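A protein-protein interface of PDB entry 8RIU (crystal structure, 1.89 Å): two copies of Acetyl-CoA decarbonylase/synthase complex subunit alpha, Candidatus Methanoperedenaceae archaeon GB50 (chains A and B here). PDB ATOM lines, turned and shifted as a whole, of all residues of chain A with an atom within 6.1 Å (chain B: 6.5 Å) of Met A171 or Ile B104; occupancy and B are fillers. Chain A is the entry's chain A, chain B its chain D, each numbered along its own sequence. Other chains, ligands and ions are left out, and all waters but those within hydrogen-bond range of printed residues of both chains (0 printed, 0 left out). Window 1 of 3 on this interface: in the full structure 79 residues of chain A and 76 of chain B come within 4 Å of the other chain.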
ATOM      1  N   PHE A  70      19.328  13.811  -9.500  1.00  0.00           N
ATOM      2  CA  PHE A  70      19.968  13.297  -8.256  1.00  0.00           C
ATOM      3  C   PHE A  70      19.015  12.998  -7.089  1.00  0.00           C
ATOM      4  O   PHE A  70      19.450  12.279  -6.190  1.00  0.00           O
ATOM      5  CB  PHE A  70      21.080  14.252  -7.820  1.00  0.00           C
ATOM      6  CG  PHE A  70      22.185  14.498  -8.814  1.00  0.00           C
ATOM      7  CD1 PHE A  70      22.227  13.829 -10.026  1.00  0.00           C
ATOM      8  CD2 PHE A  70      23.194  15.402  -8.529  1.00  0.00           C
ATOM      9  CE1 PHE A  70      23.251  14.061 -10.928  1.00  0.00           C
ATOM     10  CE2 PHE A  70      24.218  15.632  -9.431  1.00  0.00           C
ATOM     11  CZ  PHE A  70      24.244  14.963 -10.629  1.00  0.00           C
ATOM     12  N   ILE A 100      31.652  16.481  -8.769  1.00  0.00           N
ATOM     13  CA  ILE A 100      31.473  15.005  -8.688  1.00  0.00           C
ATOM     14  C   ILE A 100      32.493  14.331  -9.606  1.00  0.00           C
ATOM     15  O   ILE A 100      33.163  13.404  -9.152  1.00  0.00           O
ATOM     16  CB  ILE A 100      30.030  14.604  -9.045  1.00  0.00           C
ATOM     17  CG1 ILE A 100      29.040  15.091  -7.985  1.00  0.00           C
ATOM     18  CG2 ILE A 100      29.926  13.106  -9.272  1.00  0.00           C
ATOM     19  CD1 ILE A 100      27.638  15.277  -8.500  1.00  0.00           C
ATOM     20  N   LEU A 103      35.813  14.501  -8.075  1.00  0.00           N
ATOM     21  CA  LEU A 103      35.860  13.609  -6.921  1.00  0.00           C
ATOM     22  C   LEU A 103      36.055  12.160  -7.358  1.00  0.00           C
ATOM     23  O   LEU A 103      36.770  11.393  -6.699  1.00  0.00           O
ATOM     24  CB  LEU A 103      34.581  13.762  -6.102  1.00  0.00           C
ATOM     25  CG  LEU A 103      34.551  14.980  -5.180  1.00  0.00           C
ATOM     26  CD1 LEU A 103      33.134  15.280  -4.721  1.00  0.00           C
ATOM     27  CD2 LEU A 103      35.465  14.751  -3.976  1.00  0.00           C
ATOM     28  N   SER A 107      39.365  10.181  -6.438  1.00  0.00           N
ATOM     29  CA  SER A 107      39.272   8.904  -5.740  1.00  0.00           C
ATOM     30  C   SER A 107      40.027   7.817  -6.487  1.00  0.00           C
ATOM     31  O   SER A 107      40.641   6.939  -5.870  1.00  0.00           O
ATOM     32  CB  SER A 107      37.806   8.506  -5.569  1.00  0.00           C
ATOM     33  OG  SER A 107      37.123   9.433  -4.745  1.00  0.00           O
ATOM     34  N   GLN A 166      39.369  14.247   3.262  1.00  0.00           N
ATOM     35  CA  GLN A 166      38.870  15.376   2.481  1.00  0.00           C
ATOM     36  C   GLN A 166      37.888  14.924   1.411  1.00  0.00           C
ATOM     37  O   GLN A 166      36.899  15.612   1.137  1.00  0.00           O
ATOM     38  CB  GLN A 166      40.034  16.122   1.828  1.00  0.00           C
ATOM     39  CG  GLN A 166      40.879  16.918   2.800  1.00  0.00           C
ATOM     40  CD  GLN A 166      40.091  17.990   3.519  1.00  0.00           C
ATOM     41  OE1 GLN A 166      39.542  18.897   2.898  1.00  0.00           O
ATOM     42  NE2 GLN A 166      40.042  17.900   4.839  1.00  0.00           N
ATOM     43  N   ILE A 167      38.159  13.781   0.775  1.00  0.00           N
ATOM     44  CA  ILE A 167      37.245  13.265  -0.244  1.00  0.00           C
ATOM     45  C   ILE A 167      35.836  13.160   0.327  1.00  0.00           C
ATOM     46  O   ILE A 167      34.860  13.619  -0.282  1.00  0.00           O
ATOM     47  CB  ILE A 167      37.745  11.908  -0.776  1.00  0.00           C
ATOM     48  CG1 ILE A 167      38.946  12.104  -1.707  1.00  0.00           C
ATOM     49  CG2 ILE A 167      36.633  11.167  -1.513  1.00  0.00           C
ATOM     50  CD1 ILE A 167      39.671  10.804  -2.063  1.00  0.00           C
ATOM     51  N   ALA A 168      35.715  12.561   1.517  1.00  0.00           N
ATOM     52  CA  ALA A 168      34.407  12.388   2.142  1.00  0.00           C
ATOM     53  C   ALA A 168      33.783  13.725   2.524  1.00  0.00           C
ATOM     54  O   ALA A 168      32.558  13.882   2.464  1.00  0.00           O
ATOM     55  CB  ALA A 168      34.528  11.499   3.375  1.00  0.00           C
ATOM     56  N   GLN A 169      34.598  14.693   2.945  1.00  0.00           N
ATOM     57  CA  GLN A 169      34.060  16.011   3.264  1.00  0.00           C
ATOM     58  C   GLN A 169      33.427  16.657   2.037  1.00  0.00           C
ATOM     59  O   GLN A 169      32.305  17.170   2.101  1.00  0.00           O
ATOM     60  CB  GLN A 169      35.159  16.917   3.824  1.00  0.00           C
ATOM     61  CG  GLN A 169      35.743  16.491   5.167  1.00  0.00           C
ATOM     62  CD  GLN A 169      34.753  16.620   6.317  1.00  0.00           C
ATOM     63  OE1 GLN A 169      34.340  17.724   6.677  1.00  0.00           O
ATOM     64  NE2 GLN A 169      34.420  15.495   6.941  1.00  0.00           N
ATOM     65  N   VAL A 170      34.138  16.659   0.915  1.00  0.00           N
ATOM     66  CA  VAL A 170      33.607  17.362  -0.289  1.00  0.00           C
ATOM     67  C   VAL A 170      32.430  16.575  -0.878  1.00  0.00           C
ATOM     68  O   VAL A 170      31.464  17.202  -1.301  1.00  0.00           O
ATOM     69  CB  VAL A 170      34.713  17.631  -1.327  1.00  0.00           C
ATOM     70  CG1 VAL A 170      34.192  18.426  -2.512  1.00  0.00           C
ATOM     71  CG2 VAL A 170      35.914  18.319  -0.697  1.00  0.00           C
ATOM     72  N   MET A 171      32.523  15.250  -0.887  1.00  0.00           N
ATOM     73  CA  MET A 171      31.380  14.433  -1.364  1.00  0.00           C
ATOM     74  C   MET A 171      30.141  14.827  -0.559  1.00  0.00           C
ATOM     75  O   MET A 171      29.055  14.935  -1.149  1.00  0.00           O
ATOM     76  CB  MET A 171      31.662  12.941  -1.181  1.00  0.00           C
ATOM     77  CG  MET A 171      32.432  12.346  -2.334  1.00  0.00           C
ATOM     78  SD  MET A 171      31.377  12.204  -3.788  1.00  0.00           S
ATOM     79  CE  MET A 171      30.545  10.667  -3.402  1.00  0.00           C
ATOM     80  N   ASP A 172      30.322  15.059   0.742  1.00  0.00           N
ATOM     81  CA  ASP A 172      29.183  15.470   1.599  1.00  0.00           C
ATOM     82  C   ASP A 172      28.602  16.743   0.973  1.00  0.00           C
ATOM     83  O   ASP A 172      27.381  16.834   0.903  1.00  0.00           O
ATOM     84  CB  ASP A 172      29.682  15.610   3.039  1.00  0.00           C
ATOM     85  CG  ASP A 172      28.699  16.193   4.032  1.00  0.00           C
ATOM     86  OD1 ASP A 172      27.487  16.113   3.787  1.00  0.00           O
ATOM     87  OD2 ASP A 172      29.171  16.702   5.054  1.00  0.00           O
ATOM     88  N   SER A 173      29.458  17.638   0.473  1.00  0.00           N
ATOM     89  CA  SER A 173      29.015  18.933  -0.118  1.00  0.00           C
ATOM     90  C   SER A 173      28.139  18.738  -1.363  1.00  0.00           C
ATOM     91  O   SER A 173      27.423  19.687  -1.716  1.00  0.00           O
ATOM     92  CB  SER A 173      30.208  19.794  -0.444  1.00  0.00           C
ATOM     93  OG  SER A 173      30.708  19.507  -1.740  1.00  0.00           O
ATOM     94  N   VAL A 174      28.207  17.579  -2.017  1.00  0.00           N
ATOM     95  CA  VAL A 174      27.441  17.418  -3.287  1.00  0.00           C
ATOM     96  C   VAL A 174      26.054  16.854  -2.958  1.00  0.00           C
ATOM     97  O   VAL A 174      25.242  16.717  -3.884  1.00  0.00           O
ATOM     98  CB  VAL A 174      28.213  16.572  -4.318  1.00  0.00           C
ATOM     99  CG1 VAL A 174      29.691  16.927  -4.344  1.00  0.00           C
ATOM    100  CG2 VAL A 174      28.020  15.085  -4.101  1.00  0.00           C
ATOM    101  N   HIS A 175      25.800  16.554  -1.683  1.00  0.00           N
ATOM    102  CA  HIS A 175      24.442  16.107  -1.277  1.00  0.00           C
ATOM    103  C   HIS A 175      23.445  17.249  -1.477  1.00  0.00           C
ATOM    104  O   HIS A 175      23.819  18.426  -1.330  1.00  0.00           O
ATOM    105  CB  HIS A 175      24.419  15.601   0.170  1.00  0.00           C
ATOM    106  CG  HIS A 175      23.139  14.931   0.544  1.00  0.00           C
ATOM    107  ND1 HIS A 175      21.978  15.628   0.797  1.00  0.00           N
ATOM    108  CD2 HIS A 175      22.832  13.637   0.697  1.00  0.00           C
ATOM    109  CE1 HIS A 175      21.011  14.773   1.092  1.00  0.00           C
ATOM    110  NE2 HIS A 175      21.508  13.559   1.037  1.00  0.00           N
ATOM    111  N   THR A 176      22.208  16.903  -1.821  1.00  0.00           N
ATOM    112  CA  THR A 176      21.156  17.892  -1.984  1.00  0.00           C
ATOM    113  C   THR A 176      21.066  18.778  -0.751  1.00  0.00           C
ATOM    114  O   THR A 176      21.188  18.309   0.385  1.00  0.00           O
ATOM    115  CB  THR A 176      19.809  17.203  -2.225  1.00  0.00           C
ATOM    116  OG1 THR A 176      19.913  16.288  -3.327  1.00  0.00           O
ATOM    117  CG2 THR A 176      18.734  18.237  -2.504  1.00  0.00           C
ATOM    118  N   GLN A 178      23.074  21.543  -0.019  1.00  0.00           N
ATOM    119  CA  GLN A 178      24.370  21.947   0.513  1.00  0.00           C
ATOM    120  C   GLN A 178      24.762  23.270  -0.138  1.00  0.00           C
ATOM    121  O   GLN A 178      23.943  24.189  -0.197  1.00  0.00           O
ATOM    122  CB  GLN A 178      25.412  20.855   0.262  1.00  0.00           C
ATOM    123  CG  GLN A 178      25.168  19.584   1.061  1.00  0.00           C
ATOM    124  CD  GLN A 178      25.749  19.653   2.462  1.00  0.00           C
ATOM    125  OE1 GLN A 178      25.565  20.638   3.172  1.00  0.00           O
ATOM    126  NE2 GLN A 178      26.453  18.602   2.866  1.00  0.00           N
ATOM    127  N   THR B  99      24.894   3.524  -6.883  1.00  0.00           N
ATOM    128  CA  THR B  99      26.113   3.470  -6.087  1.00  0.00           C
ATOM    129  C   THR B  99      26.640   4.875  -5.821  1.00  0.00           C
ATOM    130  O   THR B  99      27.055   5.196  -4.699  1.00  0.00           O
ATOM    131  CB  THR B  99      27.173   2.631  -6.800  1.00  0.00           C
ATOM    132  OG1 THR B  99      26.701   1.284  -6.950  1.00  0.00           O
ATOM    133  CG2 THR B  99      28.473   2.616  -6.007  1.00  0.00           C
ATOM    134  N   ILE B 100      26.625   5.731  -6.844  1.00  0.00           N
ATOM    135  CA  ILE B 100      27.043   7.113  -6.655  1.00  0.00           C
ATOM    136  C   ILE B 100      26.126   7.804  -5.660  1.00  0.00           C
ATOM    137  O   ILE B 100      26.586   8.525  -4.768  1.00  0.00           O
ATOM    138  CB  ILE B 100      27.080   7.850  -8.005  1.00  0.00           C
ATOM    139  CG1 ILE B 100      28.251   7.341  -8.851  1.00  0.00           C
ATOM    140  CG2 ILE B 100      27.190   9.351  -7.794  1.00  0.00           C
ATOM    141  CD1 ILE B 100      28.163   7.750 -10.312  1.00  0.00           C
ATOM    142  N   ALA B 101      24.812   7.586  -5.783  1.00  0.00           N
ATOM    143  CA  ALA B 101      23.881   8.193  -4.840  1.00  0.00           C
ATOM    144  C   ALA B 101      24.143   7.693  -3.427  1.00  0.00           C
ATOM    145  O   ALA B 101      24.132   8.476  -2.470  1.00  0.00           O
ATOM    146  CB  ALA B 101      22.439   7.898  -5.252  1.00  0.00           C
ATOM    147  N   CYS B 102      24.394   6.386  -3.280  1.00  0.00           N
ATOM    148  CA  CYS B 102      24.700   5.831  -1.967  1.00  0.00           C
ATOM    149  C   CYS B 102      25.992   6.414  -1.412  1.00  0.00           C
ATOM    150  O   CYS B 102      26.073   6.749  -0.224  1.00  0.00           O
ATOM    151  CB  CYS B 102      24.792   4.310  -2.051  1.00  0.00           C
ATOM    152  SG  CYS B 102      23.191   3.491  -2.213  1.00  0.00           S
ATOM    153  N   LEU B 103      27.012   6.552  -2.262  1.00  0.00           N
ATOM    154  CA  LEU B 103      28.266   7.163  -1.837  1.00  0.00           C
ATOM    155  C   LEU B 103      28.057   8.594  -1.340  1.00  0.00           C
ATOM    156  O   LEU B 103      28.696   9.020  -0.371  1.00  0.00           O
ATOM    157  CB  LEU B 103      29.261   7.130  -2.994  1.00  0.00           C
ATOM    158  CG  LEU B 103      29.910   5.763  -3.224  1.00  0.00           C
ATOM    159  CD1 LEU B 103      30.406   5.663  -4.659  1.00  0.00           C
ATOM    160  CD2 LEU B 103      31.039   5.501  -2.231  1.00  0.00           C
ATOM    161  N   ILE B 104      27.166   9.337  -1.993  1.00  0.00           N
ATOM    162  CA  ILE B 104      26.894  10.735  -1.550  1.00  0.00           C
ATOM    163  C   ILE B 104      26.213  10.686  -0.176  1.00  0.00           C
ATOM    164  O   ILE B 104      26.593  11.488   0.692  1.00  0.00           O
ATOM    165  CB  ILE B 104      26.076  11.522  -2.594  1.00  0.00           C
ATOM    166  CG1 ILE B 104      26.921  11.903  -3.813  1.00  0.00           C
ATOM    167  CG2 ILE B 104      25.429  12.743  -1.961  1.00  0.00           C
ATOM    168  CD1 ILE B 104      26.115  12.108  -5.073  1.00  0.00           C
ATOM    169  N   GLY B 105      25.269   9.762   0.017  1.00  0.00           N
ATOM    170  CA  GLY B 105      24.634   9.632   1.316  1.00  0.00           C
ATOM    171  C   GLY B 105      25.614   9.166   2.374  1.00  0.00           C
ATOM    172  O   GLY B 105      25.702   9.747   3.459  1.00  0.00           O
ATOM    173  N   CYS B 106      26.374   8.115   2.065  1.00  0.00           N
ATOM    174  CA  CYS B 106      27.349   7.594   3.016  1.00  0.00           C
ATOM    175  C   CYS B 106      28.367   8.657   3.403  1.00  0.00           C
ATOM    176  O   CYS B 106      28.738   8.777   4.579  1.00  0.00           O
ATOM    177  CB  CYS B 106      28.058   6.377   2.418  1.00  0.00           C
ATOM    178  SG  CYS B 106      29.332   5.664   3.490  1.00  0.00           S
ATOM    179  N   SER B 107      28.839   9.429   2.421  1.00  0.00           N
ATOM    180  CA  SER B 107      29.783  10.500   2.707  1.00  0.00           C
ATOM    181  C   SER B 107      29.154  11.577   3.570  1.00  0.00           C
ATOM    182  O   SER B 107      29.841  12.199   4.384  1.00  0.00           O
ATOM    183  CB  SER B 107      30.284  11.133   1.409  1.00  0.00           C
ATOM    184  OG  SER B 107      31.265  10.326   0.788  1.00  0.00           O
ATOM    185  N   ALA B 108      27.861  11.837   3.381  1.00  0.00           N
ATOM    186  CA  ALA B 108      27.217  12.883   4.163  1.00  0.00           C
ATOM    187  C   ALA B 108      27.194  12.511   5.640  1.00  0.00           C
ATOM    188  O   ALA B 108      27.509  13.339   6.503  1.00  0.00           O
ATOM    189  CB  ALA B 108      25.806  13.136   3.632  1.00  0.00           C
ATOM    190  N   HIS B 109      26.845  11.262   5.947  1.00  0.00           N
ATOM    191  CA  HIS B 109      26.803  10.824   7.336  1.00  0.00           C
ATOM    192  C   HIS B 109      28.203  10.669   7.913  1.00  0.00           C
ATOM    193  O   HIS B 109      28.455  11.073   9.052  1.00  0.00           O
ATOM    194  CB  HIS B 109      26.040   9.507   7.436  1.00  0.00           C
ATOM    195  CG  HIS B 109      24.589   9.627   7.095  1.00  0.00           C
ATOM    196  ND1 HIS B 109      23.957   8.772   6.216  1.00  0.00           N
ATOM    197  CD2 HIS B 109      23.644  10.500   7.517  1.00  0.00           C
ATOM    198  CE1 HIS B 109      22.686   9.114   6.110  1.00  0.00           C
ATOM    199  NE2 HIS B 109      22.469  10.157   6.892  1.00  0.00           N
ATOM    200  N   ILE B 167      35.267   4.482   1.198  1.00  0.00           N
ATOM    201  CA  ILE B 167      34.530   5.379   0.312  1.00  0.00           C
ATOM    202  C   ILE B 167      35.352   5.686  -0.932  1.00  0.00           C
ATOM    203  O   ILE B 167      34.827   5.710  -2.051  1.00  0.00           O
ATOM    204  CB  ILE B 167      34.139   6.670   1.059  1.00  0.00           C
ATOM    205  CG1 ILE B 167      32.915   6.435   1.947  1.00  0.00           C
ATOM    206  CG2 ILE B 167      33.853   7.813   0.068  1.00  0.00           C
ATOM    207  CD1 ILE B 167      32.686   7.535   2.969  1.00  0.00           C
ATOM    208  N   MET B 171      34.333   4.734  -4.710  1.00  0.00           N
ATOM    209  CA  MET B 171      34.215   5.875  -5.656  1.00  0.00           C
ATOM    210  C   MET B 171      35.118   5.600  -6.859  1.00  0.00           C
ATOM    211  O   MET B 171      34.698   5.886  -7.986  1.00  0.00           O
ATOM    212  CB  MET B 171      34.616   7.186  -4.980  1.00  0.00           C
ATOM    213  CG  MET B 171      33.442   7.926  -4.388  1.00  0.00           C
ATOM    214  SD  MET B 171      32.623   8.932  -5.641  1.00  0.00           S
ATOM    215  CE  MET B 171      33.743  10.328  -5.699  1.00  0.00           C
ATOM    216  N   VAL B 192      28.456   0.192   0.341  1.00  0.00           N
ATOM    217  CA  VAL B 192      28.365   1.593   0.749  1.00  0.00           C
ATOM    218  C   VAL B 192      27.247   1.771   1.770  1.00  0.00           C
ATOM    219  O   VAL B 192      27.378   2.546   2.726  1.00  0.00           O
ATOM    220  CB  VAL B 192      28.163   2.502  -0.481  1.00  0.00           C
ATOM    221  CG1 VAL B 192      28.029   3.955  -0.052  1.00  0.00           C
ATOM    222  CG2 VAL B 192      29.328   2.352  -1.466  1.00  0.00           C
ATOM    223  N   GLN B 621      19.897  11.571  -1.153  1.00  0.00           N
ATOM    224  CA  GLN B 621      20.913  10.540  -1.345  1.00  0.00           C
ATOM    225  C   GLN B 621      21.180   9.798  -0.043  1.00  0.00           C
ATOM    226  O   GLN B 621      21.425   8.585  -0.046  1.00  0.00           O
ATOM    227  CB  GLN B 621      22.205  11.165  -1.869  1.00  0.00           C
ATOM    228  CG  GLN B 621      22.084  11.833  -3.227  1.00  0.00           C
ATOM    229  CD  GLN B 621      21.620  13.266  -3.119  1.00  0.00           C
ATOM    230  OE1 GLN B 621      21.932  13.963  -2.148  1.00  0.00           O
ATOM    231  NE2 GLN B 621      20.851  13.713  -4.104  1.00  0.00           N
ATOM    232  N   LYS B 622      21.139  10.523   1.076  1.00  0.00           N
ATOM    233  CA  LYS B 622      21.192   9.894   2.388  1.00  0.00           C
ATOM    234  C   LYS B 622      20.104   8.839   2.541  1.00  0.00           C
ATOM    235  O   LYS B 622      20.338   7.776   3.127  1.00  0.00           O
ATOM    236  CB  LYS B 622      21.063  10.966   3.473  1.00  0.00           C
ATOM    237  CG  LYS B 622      22.377  11.665   3.785  1.00  0.00           C
ATOM    238  CD  LYS B 622      22.229  12.700   4.898  1.00  0.00           C
ATOM    239  CE  LYS B 622      21.416  13.910   4.459  1.00  0.00           C
ATOM    240  NZ  LYS B 622      21.028  14.771   5.621  1.00  0.00           N
ATOM    241  N   SER B 625      21.269   5.755   0.723  1.00  0.00           N
ATOM    242  CA  SER B 625      22.299   5.023   1.456  1.00  0.00           C
ATOM    243  C   SER B 625      21.732   4.383   2.719  1.00  0.00           C
ATOM    244  O   SER B 625      22.166   3.289   3.101  1.00  0.00           O
ATOM    245  CB  SER B 625      23.483   5.944   1.785  1.00  0.00           C
ATOM    246  OG  SER B 625      23.112   7.071   2.569  1.00  0.00           O
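The backbone carbonyl oxygen of Phe A70 is in hydrogen-bond range of the side-chain amide nitrogen of Gln B621, 2.9 Å away.
NE2 of His A175 sits close to OE1 of Gln B621 (3.2 Å).
A ring nitrogen (NE2) of His A175 is in hydrogen-bond range of the backbone NH (N) of Lys B622, at 3.1 Å.
The side-chain hydroxyl (OG1) of Thr A176 is in hydrogen-bond range of the side-chain amide nitrogen (NE2) of Gln B621.
OG of Ser A107 is in hydrogen-bond range of O of Leu A103, 2.8 Å away.
The backbone carbonyl oxygen (O) of Asp A172 sits at hydrogen-bond distance from the side-chain amide nitrogen (NE2) of Gln A178 (2.8 Å).
The side-chain hydroxyl (OG) of Ser B107 lies within hydrogen-bond range of the backbone carbonyl oxygen (O) of Leu B103 (3.1 Å).
OG of Ser B625 is in hydrogen-bond range of O of Gln B621, 3.5 Å away.
The backbone carbonyl oxygen (O) of Lys B622 sits at hydrogen-bond distance from the side-chain hydroxyl (OG) of Ser B625, at 2.9 Å.
Among the printed residues, pairs that only touch across the chains: Asp A172 with Ala B108, Met A171 with Ser B107, Leu A103 with Met B171, Ser A107 with Met B171, Val A174 with Ile B104, Met A171 with Met B171, His A175 with Ile B104, Asp A172 with Ser B107, Ala A168 with Ser B107, Met A171 with Leu B103 and Met A171 with Ile B104.
Met A171 touches four residues of chain B.
Printed residues of chain A within 4 Å of Ile B104: Met A171 (3.9 Å), Val A174 (3.4 Å) and His A175 (3.6 Å).
Of the printed residues of chain B, Val A174 touches Ile B104.
Printed residues of chain A within 4 Å of Leu B103: Met A171 (3.8 Å).
Printed residues of chain B within 4 Å of Asp A172: Ser B107 and Ala B108.
The nearest printed residue of chain A that does not touch Ser B107 is Ile A167 (5.0 Å).
Of the 16 printed residues of chain A, 9 touch a printed residue of chain B.
Hydrophobic or aromatic side chains of chain A that line the printed part of chain B: Phe A70, Leu A103, Met A171, Val A174 and His A175.
Leu A103 touches Met B171, and with the chains exchanged Met A171 touches Leu B103.
Ser A107 touches Met B171, and with the chains exchanged Met A171 touches Ser B107.
Met B171 touches its own counterpart, Met A171.
Positions printed for both chains: 100, 103, 107, 167 and 171.
Of the 15 pairs that touch across the chains among the printed residues, 5 have their exchanged pair printed and touching as well.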
